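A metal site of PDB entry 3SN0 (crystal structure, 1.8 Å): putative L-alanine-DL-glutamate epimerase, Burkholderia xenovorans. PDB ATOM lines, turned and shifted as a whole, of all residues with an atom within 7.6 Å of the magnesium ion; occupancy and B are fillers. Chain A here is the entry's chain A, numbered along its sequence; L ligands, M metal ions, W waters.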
ATOM      1  N   PHE A  41      -5.878  21.485 -11.452  1.00  0.00           N
ATOM      2  CA  PHE A  41      -5.600  22.901 -11.682  1.00  0.00           C
ATOM      3  C   PHE A  41      -6.565  23.767 -10.871  1.00  0.00           C
ATOM      4  O   PHE A  41      -7.315  24.577 -11.411  1.00  0.00           O
ATOM      5  CB  PHE A  41      -5.644  23.209 -13.177  1.00  0.00           C
ATOM      6  CG  PHE A  41      -4.936  24.485 -13.572  1.00  0.00           C
ATOM      7  CD1 PHE A  41      -3.601  24.697 -13.198  1.00  0.00           C
ATOM      8  CD2 PHE A  41      -5.576  25.453 -14.314  1.00  0.00           C
ATOM      9  CE1 PHE A  41      -2.940  25.864 -13.572  1.00  0.00           C
ATOM     10  CE2 PHE A  41      -4.918  26.626 -14.701  1.00  0.00           C
ATOM     11  CZ  PHE A  41      -3.595  26.826 -14.329  1.00  0.00           C
ATOM     12  N   TYR A 122       1.713  25.314 -30.660  1.00  0.00           N
ATOM     13  CA  TYR A 122       2.947  25.509 -29.905  1.00  0.00           C
ATOM     14  C   TYR A 122       3.146  24.371 -28.914  1.00  0.00           C
ATOM     15  O   TYR A 122       2.182  23.787 -28.387  1.00  0.00           O
ATOM     16  CB  TYR A 122       2.998  26.861 -29.224  1.00  0.00           C
ATOM     17  CG  TYR A 122       2.030  27.118 -28.100  1.00  0.00           C
ATOM     18  CD1 TYR A 122       2.371  26.806 -26.780  1.00  0.00           C
ATOM     19  CD2 TYR A 122       0.811  27.748 -28.333  1.00  0.00           C
ATOM     20  CE1 TYR A 122       1.498  27.076 -25.733  1.00  0.00           C
ATOM     21  CE2 TYR A 122      -0.069  28.032 -27.278  1.00  0.00           C
ATOM     22  CZ  TYR A 122       0.305  27.709 -25.986  1.00  0.00           C
ATOM     23  OH  TYR A 122      -0.546  27.971 -24.931  1.00  0.00           O
ATOM     24  N   SER A 124       3.869  23.400 -25.571  1.00  0.00           N
ATOM     25  CA  SER A 124       3.650  24.061 -24.288  1.00  0.00           C
ATOM     26  C   SER A 124       4.492  23.437 -23.191  1.00  0.00           C
ATOM     27  O   SER A 124       5.021  22.331 -23.339  1.00  0.00           O
ATOM     28  CB  SER A 124       2.162  23.988 -23.949  1.00  0.00           C
ATOM     29  OG  SER A 124       1.851  24.917 -22.926  1.00  0.00           O
ATOM     30  N   HIS A 125       4.599  24.124 -22.060  1.00  0.00           N
ATOM     31  CA  HIS A 125       5.362  23.624 -20.918  1.00  0.00           C
ATOM     32  C   HIS A 125       6.732  23.109 -21.349  1.00  0.00           C
ATOM     33  O   HIS A 125       7.132  21.995 -21.034  1.00  0.00           O
ATOM     34  CB  HIS A 125       4.549  22.564 -20.173  1.00  0.00           C
ATOM     35  CG  HIS A 125       3.192  23.071 -19.766  1.00  0.00           C
ATOM     36  ND1 HIS A 125       2.059  22.798 -20.500  1.00  0.00           N
ATOM     37  CD2 HIS A 125       2.812  23.912 -18.778  1.00  0.00           C
ATOM     38  CE1 HIS A 125       1.033  23.438 -19.954  1.00  0.00           C
ATOM     39  NE2 HIS A 125       1.461  24.113 -18.903  1.00  0.00           N
ATOM     40  N   LYS A 163       6.379  27.375 -25.377  1.00  0.00           N
ATOM     41  CA  LYS A 163       5.997  28.210 -24.231  1.00  0.00           C
ATOM     42  C   LYS A 163       6.657  27.774 -22.950  1.00  0.00           C
ATOM     43  O   LYS A 163       6.572  26.598 -22.556  1.00  0.00           O
ATOM     44  CB  LYS A 163       4.483  28.245 -24.035  1.00  0.00           C
ATOM     45  CG  LYS A 163       4.031  29.337 -23.063  1.00  0.00           C
ATOM     46  CD  LYS A 163       2.521  29.583 -23.101  1.00  0.00           C
ATOM     47  CE  LYS A 163       1.741  28.538 -22.315  1.00  0.00           C
ATOM     48  NZ  LYS A 163       0.281  28.655 -22.586  1.00  0.00           N
ATOM     49  N   ASN A 165       7.709  29.097 -18.682  1.00  0.00           N
ATOM     50  CA  ASN A 165       7.161  29.776 -17.474  1.00  0.00           C
ATOM     51  C   ASN A 165       8.343  30.438 -16.754  1.00  0.00           C
ATOM     52  O   ASN A 165       9.309  30.790 -17.417  1.00  0.00           O
ATOM     53  CB  ASN A 165       6.418  28.745 -16.594  1.00  0.00           C
ATOM     54  CG  ASN A 165       5.246  28.092 -17.319  1.00  0.00           C
ATOM     55  OD1 ASN A 165       5.411  27.131 -18.088  1.00  0.00           O
ATOM     56  ND2 ASN A 165       4.019  28.598 -17.051  1.00  0.00           N
ATOM     57  N   LEU A 218       5.901  33.339 -23.385  1.00  0.00           N
ATOM     58  CA  LEU A 218       6.239  33.402 -21.948  1.00  0.00           C
ATOM     59  C   LEU A 218       4.952  33.462 -21.131  1.00  0.00           C
ATOM     60  O   LEU A 218       4.177  34.390 -21.297  1.00  0.00           O
ATOM     61  CB  LEU A 218       7.085  34.630 -21.636  1.00  0.00           C
ATOM     62  CG  LEU A 218       7.452  34.894 -20.171  1.00  0.00           C
ATOM     63  CD1 LEU A 218       8.201  33.688 -19.551  1.00  0.00           C
ATOM     64  CD2 LEU A 218       8.246  36.192 -20.046  1.00  0.00           C
ATOM     65  N   ASP A 219       4.735  32.469 -20.278  1.00  0.00           N
ATOM     66  CA  ASP A 219       3.554  32.448 -19.419  1.00  0.00           C
ATOM     67  C   ASP A 219       3.954  32.835 -17.999  1.00  0.00           C
ATOM     68  O   ASP A 219       4.752  32.146 -17.363  1.00  0.00           O
ATOM     69  CB  ASP A 219       2.899  31.065 -19.454  1.00  0.00           C
ATOM     70  CG  ASP A 219       1.462  31.079 -18.996  1.00  0.00           C
ATOM     71  OD1 ASP A 219       1.087  31.983 -18.210  1.00  0.00           O
ATOM     72  OD2 ASP A 219       0.704  30.162 -19.416  1.00  0.00           O
ATOM     73  N   LEU A 220       3.367  33.911 -17.501  1.00  0.00           N
ATOM     74  CA  LEU A 220       3.611  34.398 -16.159  1.00  0.00           C
ATOM     75  C   LEU A 220       2.494  34.014 -15.185  1.00  0.00           C
ATOM     76  O   LEU A 220       2.586  34.298 -13.989  1.00  0.00           O
ATOM     77  CB  LEU A 220       3.784  35.919 -16.197  1.00  0.00           C
ATOM     78  CG  LEU A 220       4.882  36.472 -17.118  1.00  0.00           C
ATOM     79  CD1 LEU A 220       4.854  37.994 -17.129  1.00  0.00           C
ATOM     80  CD2 LEU A 220       6.257  35.953 -16.728  1.00  0.00           C
ATOM     81  N   ASN A 221       1.470  33.325 -15.687  1.00  0.00           N
ATOM     82  CA  ASN A 221       0.311  32.914 -14.901  1.00  0.00           C
ATOM     83  C   ASN A 221      -0.177  34.046 -13.966  1.00  0.00           C
ATOM     84  O   ASN A 221      -0.336  35.195 -14.409  1.00  0.00           O
ATOM     85  CB  ASN A 221       0.619  31.592 -14.173  1.00  0.00           C
ATOM     86  CG  ASN A 221       1.047  30.491 -15.112  1.00  0.00           C
ATOM     87  OD1 ASN A 221       2.232  30.286 -15.346  1.00  0.00           O
ATOM     88  ND2 ASN A 221       0.077  29.778 -15.676  1.00  0.00           N
ATOM     89  N   TRP A 243       4.048  36.008 -27.414  1.00  0.00           N
ATOM     90  CA  TRP A 243       3.167  36.684 -26.482  1.00  0.00           C
ATOM     91  C   TRP A 243       3.670  36.500 -25.070  1.00  0.00           C
ATOM     92  O   TRP A 243       4.507  35.610 -24.803  1.00  0.00           O
ATOM     93  CB  TRP A 243       1.708  36.238 -26.600  1.00  0.00           C
ATOM     94  CG  TRP A 243       1.249  34.898 -26.056  1.00  0.00           C
ATOM     95  CD1 TRP A 243       1.530  34.367 -24.837  1.00  0.00           C
ATOM     96  CD2 TRP A 243       0.360  33.964 -26.697  1.00  0.00           C
ATOM     97  NE1 TRP A 243       0.893  33.163 -24.678  1.00  0.00           N
ATOM     98  CE2 TRP A 243       0.155  32.898 -25.810  1.00  0.00           C
ATOM     99  CE3 TRP A 243      -0.295  33.947 -27.934  1.00  0.00           C
ATOM    100  CZ2 TRP A 243      -0.654  31.809 -26.118  1.00  0.00           C
ATOM    101  CZ3 TRP A 243      -1.085  32.856 -28.247  1.00  0.00           C
ATOM    102  CH2 TRP A 243      -1.262  31.808 -27.341  1.00  0.00           C
ATOM    103  N   GLU A 245       1.830  35.885 -21.468  1.00  0.00           N
ATOM    104  CA  GLU A 245       0.567  35.421 -20.942  1.00  0.00           C
ATOM    105  C   GLU A 245       0.461  35.801 -19.467  1.00  0.00           C
ATOM    106  O   GLU A 245       1.347  35.467 -18.678  1.00  0.00           O
ATOM    107  CB  GLU A 245       0.496  33.897 -21.110  1.00  0.00           C
ATOM    108  CG  GLU A 245      -0.888  33.277 -21.065  1.00  0.00           C
ATOM    109  CD  GLU A 245      -0.884  31.807 -21.487  1.00  0.00           C
ATOM    110  OE1 GLU A 245      -1.709  31.065 -20.921  1.00  0.00           O
ATOM    111  OE2 GLU A 245      -0.072  31.401 -22.354  1.00  0.00           O
ATOM    112  N   ILE A 246      -0.620  36.479 -19.106  1.00  0.00           N
ATOM    113  CA  ILE A 246      -0.808  37.043 -17.741  1.00  0.00           C
ATOM    114  C   ILE A 246      -2.259  36.788 -17.346  1.00  0.00           C
ATOM    115  O   ILE A 246      -3.192  37.295 -17.985  1.00  0.00           O
ATOM    116  CB  ILE A 246      -0.561  38.568 -17.736  1.00  0.00           C
ATOM    117  CG1 ILE A 246       0.897  38.872 -18.085  1.00  0.00           C
ATOM    118  CG2 ILE A 246      -0.900  39.179 -16.333  1.00  0.00           C
ATOM    119  CD1 ILE A 246       1.176  40.363 -18.343  1.00  0.00           C
ATOM    120  N   ASP A 247      -2.458  35.992 -16.306  1.00  0.00           N
ATOM    121  CA  ASP A 247      -3.785  35.810 -15.742  1.00  0.00           C
ATOM    122  C   ASP A 247      -4.054  36.856 -14.686  1.00  0.00           C
ATOM    123  O   ASP A 247      -3.205  37.140 -13.816  1.00  0.00           O
ATOM    124  CB  ASP A 247      -3.918  34.415 -15.165  1.00  0.00           C
ATOM    125  CG  ASP A 247      -3.793  33.363 -16.209  1.00  0.00           C
ATOM    126  OD1 ASP A 247      -4.657  33.368 -17.137  1.00  0.00           O
ATOM    127  OD2 ASP A 247      -2.837  32.555 -16.119  1.00  0.00           O
ATOM    128  N   SER A 266      -1.588  37.813 -23.860  1.00  0.00           N
ATOM    129  CA  SER A 266      -2.661  36.841 -23.833  1.00  0.00           C
ATOM    130  C   SER A 266      -3.150  36.663 -22.403  1.00  0.00           C
ATOM    131  O   SER A 266      -2.417  36.871 -21.426  1.00  0.00           O
ATOM    132  CB  SER A 266      -2.255  35.486 -24.395  1.00  0.00           C
ATOM    133  OG  SER A 266      -1.147  34.980 -23.720  1.00  0.00           O
ATOM    134  N   SER A 267      -4.409  36.279 -22.294  1.00  0.00           N
ATOM    135  CA  SER A 267      -5.026  35.999 -20.999  1.00  0.00           C
ATOM    136  C   SER A 267      -6.301  35.194 -21.217  1.00  0.00           C
ATOM    137  O   SER A 267      -6.674  34.859 -22.355  1.00  0.00           O
ATOM    138  CB  SER A 267      -5.361  37.310 -20.265  1.00  0.00           C
ATOM    139  OG  SER A 267      -5.586  37.141 -18.862  1.00  0.00           O
ATOM    140  N   CYS A 268      -6.964  34.923 -20.099  1.00  0.00           N
ATOM    141  CA  CYS A 268      -8.367  34.528 -20.021  1.00  0.00           C
ATOM    142  C   CYS A 268      -8.580  33.029 -19.868  1.00  0.00           C
ATOM    143  O   CYS A 268      -9.728  32.605 -19.833  1.00  0.00           O
ATOM    144  CB  CYS A 268      -9.201  35.018 -21.192  1.00  0.00           C
ATOM    145  SG  CYS A 268      -9.115  36.798 -21.510  1.00  0.00           S
ATOM    146  N   GLU A 269      -7.513  32.249 -19.756  1.00  0.00           N
ATOM    147  CA  GLU A 269      -7.652  30.790 -19.695  1.00  0.00           C
ATOM    148  C   GLU A 269      -8.533  30.283 -18.558  1.00  0.00           C
ATOM    149  O   GLU A 269      -8.967  29.130 -18.600  1.00  0.00           O
ATOM    150  CB  GLU A 269      -6.295  30.090 -19.621  1.00  0.00           C
ATOM    151  CG  GLU A 269      -5.621  30.136 -18.245  1.00  0.00           C
ATOM    152  CD  GLU A 269      -4.194  29.635 -18.265  1.00  0.00           C
ATOM    153  OE1 GLU A 269      -3.771  28.962 -17.280  1.00  0.00           O
ATOM    154  OE2 GLU A 269      -3.493  29.885 -19.265  1.00  0.00           O
ATOM    155  N   THR A 270      -8.723  31.093 -17.505  1.00  0.00           N
ATOM    156  CA  THR A 270      -9.476  30.639 -16.337  1.00  0.00           C
ATOM    157  C   THR A 270     -10.906  31.186 -16.310  1.00  0.00           C
ATOM    158  O   THR A 270     -11.606  31.015 -15.296  1.00  0.00           O
ATOM    159  CB  THR A 270      -8.770  31.036 -15.023  1.00  0.00           C
ATOM    160  OG1 THR A 270      -8.815  32.453 -14.858  1.00  0.00           O
ATOM    161  CG2 THR A 270      -7.309  30.510 -15.022  1.00  0.00           C
ATOM    162  N   ILE A 290      -7.296  33.317 -24.478  1.00  0.00           N
ATOM    163  CA  ILE A 290      -7.235  31.884 -24.255  1.00  0.00           C
ATOM    164  C   ILE A 290      -8.606  31.403 -23.777  1.00  0.00           C
ATOM    165  O   ILE A 290      -9.163  31.963 -22.832  1.00  0.00           O
ATOM    166  CB  ILE A 290      -6.169  31.511 -23.195  1.00  0.00           C
ATOM    167  CG1 ILE A 290      -4.798  32.099 -23.557  1.00  0.00           C
ATOM    168  CG2 ILE A 290      -6.055  29.983 -23.053  1.00  0.00           C
ATOM    169  CD1 ILE A 290      -4.330  31.748 -24.973  1.00  0.00           C
ATOM    170  N   HIS A 318      -7.071  26.248 -24.513  1.00  0.00           N
ATOM    171  CA  HIS A 318      -6.242  25.845 -23.395  1.00  0.00           C
ATOM    172  C   HIS A 318      -6.176  24.324 -23.439  1.00  0.00           C
ATOM    173  O   HIS A 318      -7.178  23.649 -23.300  1.00  0.00           O
ATOM    174  CB  HIS A 318      -6.906  26.320 -22.109  1.00  0.00           C
ATOM    175  CG  HIS A 318      -5.989  26.389 -20.925  1.00  0.00           C
ATOM    176  ND1 HIS A 318      -6.463  26.413 -19.641  1.00  0.00           N
ATOM    177  CD2 HIS A 318      -4.643  26.536 -20.840  1.00  0.00           C
ATOM    178  CE1 HIS A 318      -5.453  26.524 -18.799  1.00  0.00           C
ATOM    179  NE2 HIS A 318      -4.338  26.625 -19.502  1.00  0.00           N
ATOM    180  N   PHE A 320      -3.600  21.184 -22.231  1.00  0.00           N
ATOM    181  CA  PHE A 320      -2.394  20.691 -21.545  1.00  0.00           C
ATOM    182  C   PHE A 320      -2.717  19.467 -20.687  1.00  0.00           C
ATOM    183  O   PHE A 320      -2.176  19.278 -19.605  1.00  0.00           O
ATOM    184  CB  PHE A 320      -1.754  21.802 -20.697  1.00  0.00           C
ATOM    185  CG  PHE A 320      -2.597  22.274 -19.534  1.00  0.00           C
ATOM    186  CD1 PHE A 320      -2.171  22.097 -18.223  1.00  0.00           C
ATOM    187  CD2 PHE A 320      -3.773  22.974 -19.751  1.00  0.00           C
ATOM    188  CE1 PHE A 320      -2.955  22.548 -17.147  1.00  0.00           C
ATOM    189  CE2 PHE A 320      -4.560  23.412 -18.681  1.00  0.00           C
ATOM    190  CZ  PHE A 320      -4.142  23.205 -17.390  1.00  0.00           C
ATOM    191  N   GLU A 343      -2.482  25.301 -28.371  1.00  0.00           N
ATOM    192  CA  GLU A 343      -1.554  24.784 -27.383  1.00  0.00           C
ATOM    193  C   GLU A 343      -1.568  23.277 -27.420  1.00  0.00           C
ATOM    194  O   GLU A 343      -2.618  22.652 -27.606  1.00  0.00           O
ATOM    195  CB  GLU A 343      -2.008  25.231 -25.995  1.00  0.00           C
ATOM    196  CG  GLU A 343      -1.105  24.751 -24.881  1.00  0.00           C
ATOM    197  CD  GLU A 343      -1.580  25.120 -23.503  1.00  0.00           C
ATOM    198  OE1 GLU A 343      -2.760  25.506 -23.326  1.00  0.00           O
ATOM    199  OE2 GLU A 343      -0.762  25.004 -22.586  1.00  0.00           O
HETATM  200  O1  LIG L   1       2.769  26.861 -12.636  1.00  0.00           O
HETATM  201  C1  LIG L   1       1.826  26.067 -12.902  1.00  0.00           C
HETATM  202  O2  LIG L   1       1.364  25.305 -12.007  1.00  0.00           O
HETATM  203  C2  LIG L   1       1.253  25.951 -14.260  1.00  0.00           C
HETATM  204  C3  LIG L   1       1.672  26.720 -15.279  1.00  0.00           C
HETATM  205  C4  LIG L   1       1.071  26.598 -16.626  1.00  0.00           C
HETATM  206  O3  LIG L   1       0.224  25.677 -16.829  1.00  0.00           O
HETATM  207  O4  LIG L   1       1.411  27.411 -17.527  1.00  0.00           O
HETATM  208 MG    MG M   1      -1.473  30.009 -19.339  1.00  0.00          MG
HETATM  209  O   HOH W   1      -1.228  28.499 -18.058  1.00  0.00           O
HETATM  210  O   HOH W   2      -1.473  31.527 -18.040  1.00  0.00           O
HETATM  211  O   HOH W   3      -1.417  28.479 -20.895  1.00  0.00           O
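The side-chain amino group (NZ) of Lys 163 is in salt-bridge range of the side-chain carboxylate (OE2) of Glu 245, 2.8 Å away. The side-chain carboxylate (OE2) of Glu 343 lies within salt-bridge range of the side-chain amino group (NZ) of Lys 163 (3.8 Å). The backbone NH (N) of Leu 220 sits at hydrogen-bond distance from the backbone carbonyl oxygen (O) of Glu 245. O of Lys 163 lies within hydrogen-bond range of N of His 125. The side-chain carboxylate of Glu 245 lies within hydrogen-bond range of the indole nitrogen of Trp 243, 3.1 Å away. A ring nitrogen (NE2) of His 318 sits close to the side-chain carboxylate (OE1) of Glu 269 (3.3 Å). OH of Tyr 122 is in hydrogen-bond range of NZ of Lys 163. O of Leu 218 lies within hydrogen-bond range of N of Glu 245 (2.8 Å).
NZ of Lys 163 touches the magnesium ion, 3.9 Å away. Asn 221 touches the magnesium ion (ND2 to MG, 3.98 Å). Of the 23 residues printed, 5 come within 4 Å of the magnesium ion. Along chain A the residues within 4 Å of the magnesium ion span positions 163 to 269. The nearest printed residue that does not touch the magnesium ion is Asp 247 (4.3 Å).
The side-chain carboxylate (OE1) of Glu 245 binds the magnesium ion. The magnesium ion is bound by water W1, at 2.0 Å. Water W2 is bound to the magnesium ion, at 2.0 Å. OE2 of Glu 269 binds the magnesium ion (2.0 Å). The magnesium ion is bound by water W3 (2.2 Å). OD2 of Asp 219 binds the magnesium ion, 2.2 Å away. The magnesium ion has six donor atoms within binding distance.
Water W1 lies within hydrogen-bond range of the side-chain carboxylate of Glu 269 (2.7 Å), an oxygen (O4) of the ligand (2.9 Å) and the side-chain amide nitrogen of Asn 221 (3.0 Å). Water W2 lies within hydrogen-bond range of OD2 of Asp 247 (2.6 Å), OD1 of Asp 219 (2.6 Å) and ND2 of Asn 221 (3.3 Å).
NE2 of His 125 is in hydrogen-bond range of O3 of the ligand. An oxygen (O4) of the ligand lies within hydrogen-bond range of the side-chain amide nitrogen of Asn 165 (2.9 Å). The side-chain amide nitrogen of Asn 221 lies within hydrogen-bond range of an oxygen (O4) of the ligand, 3.3 Å away.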
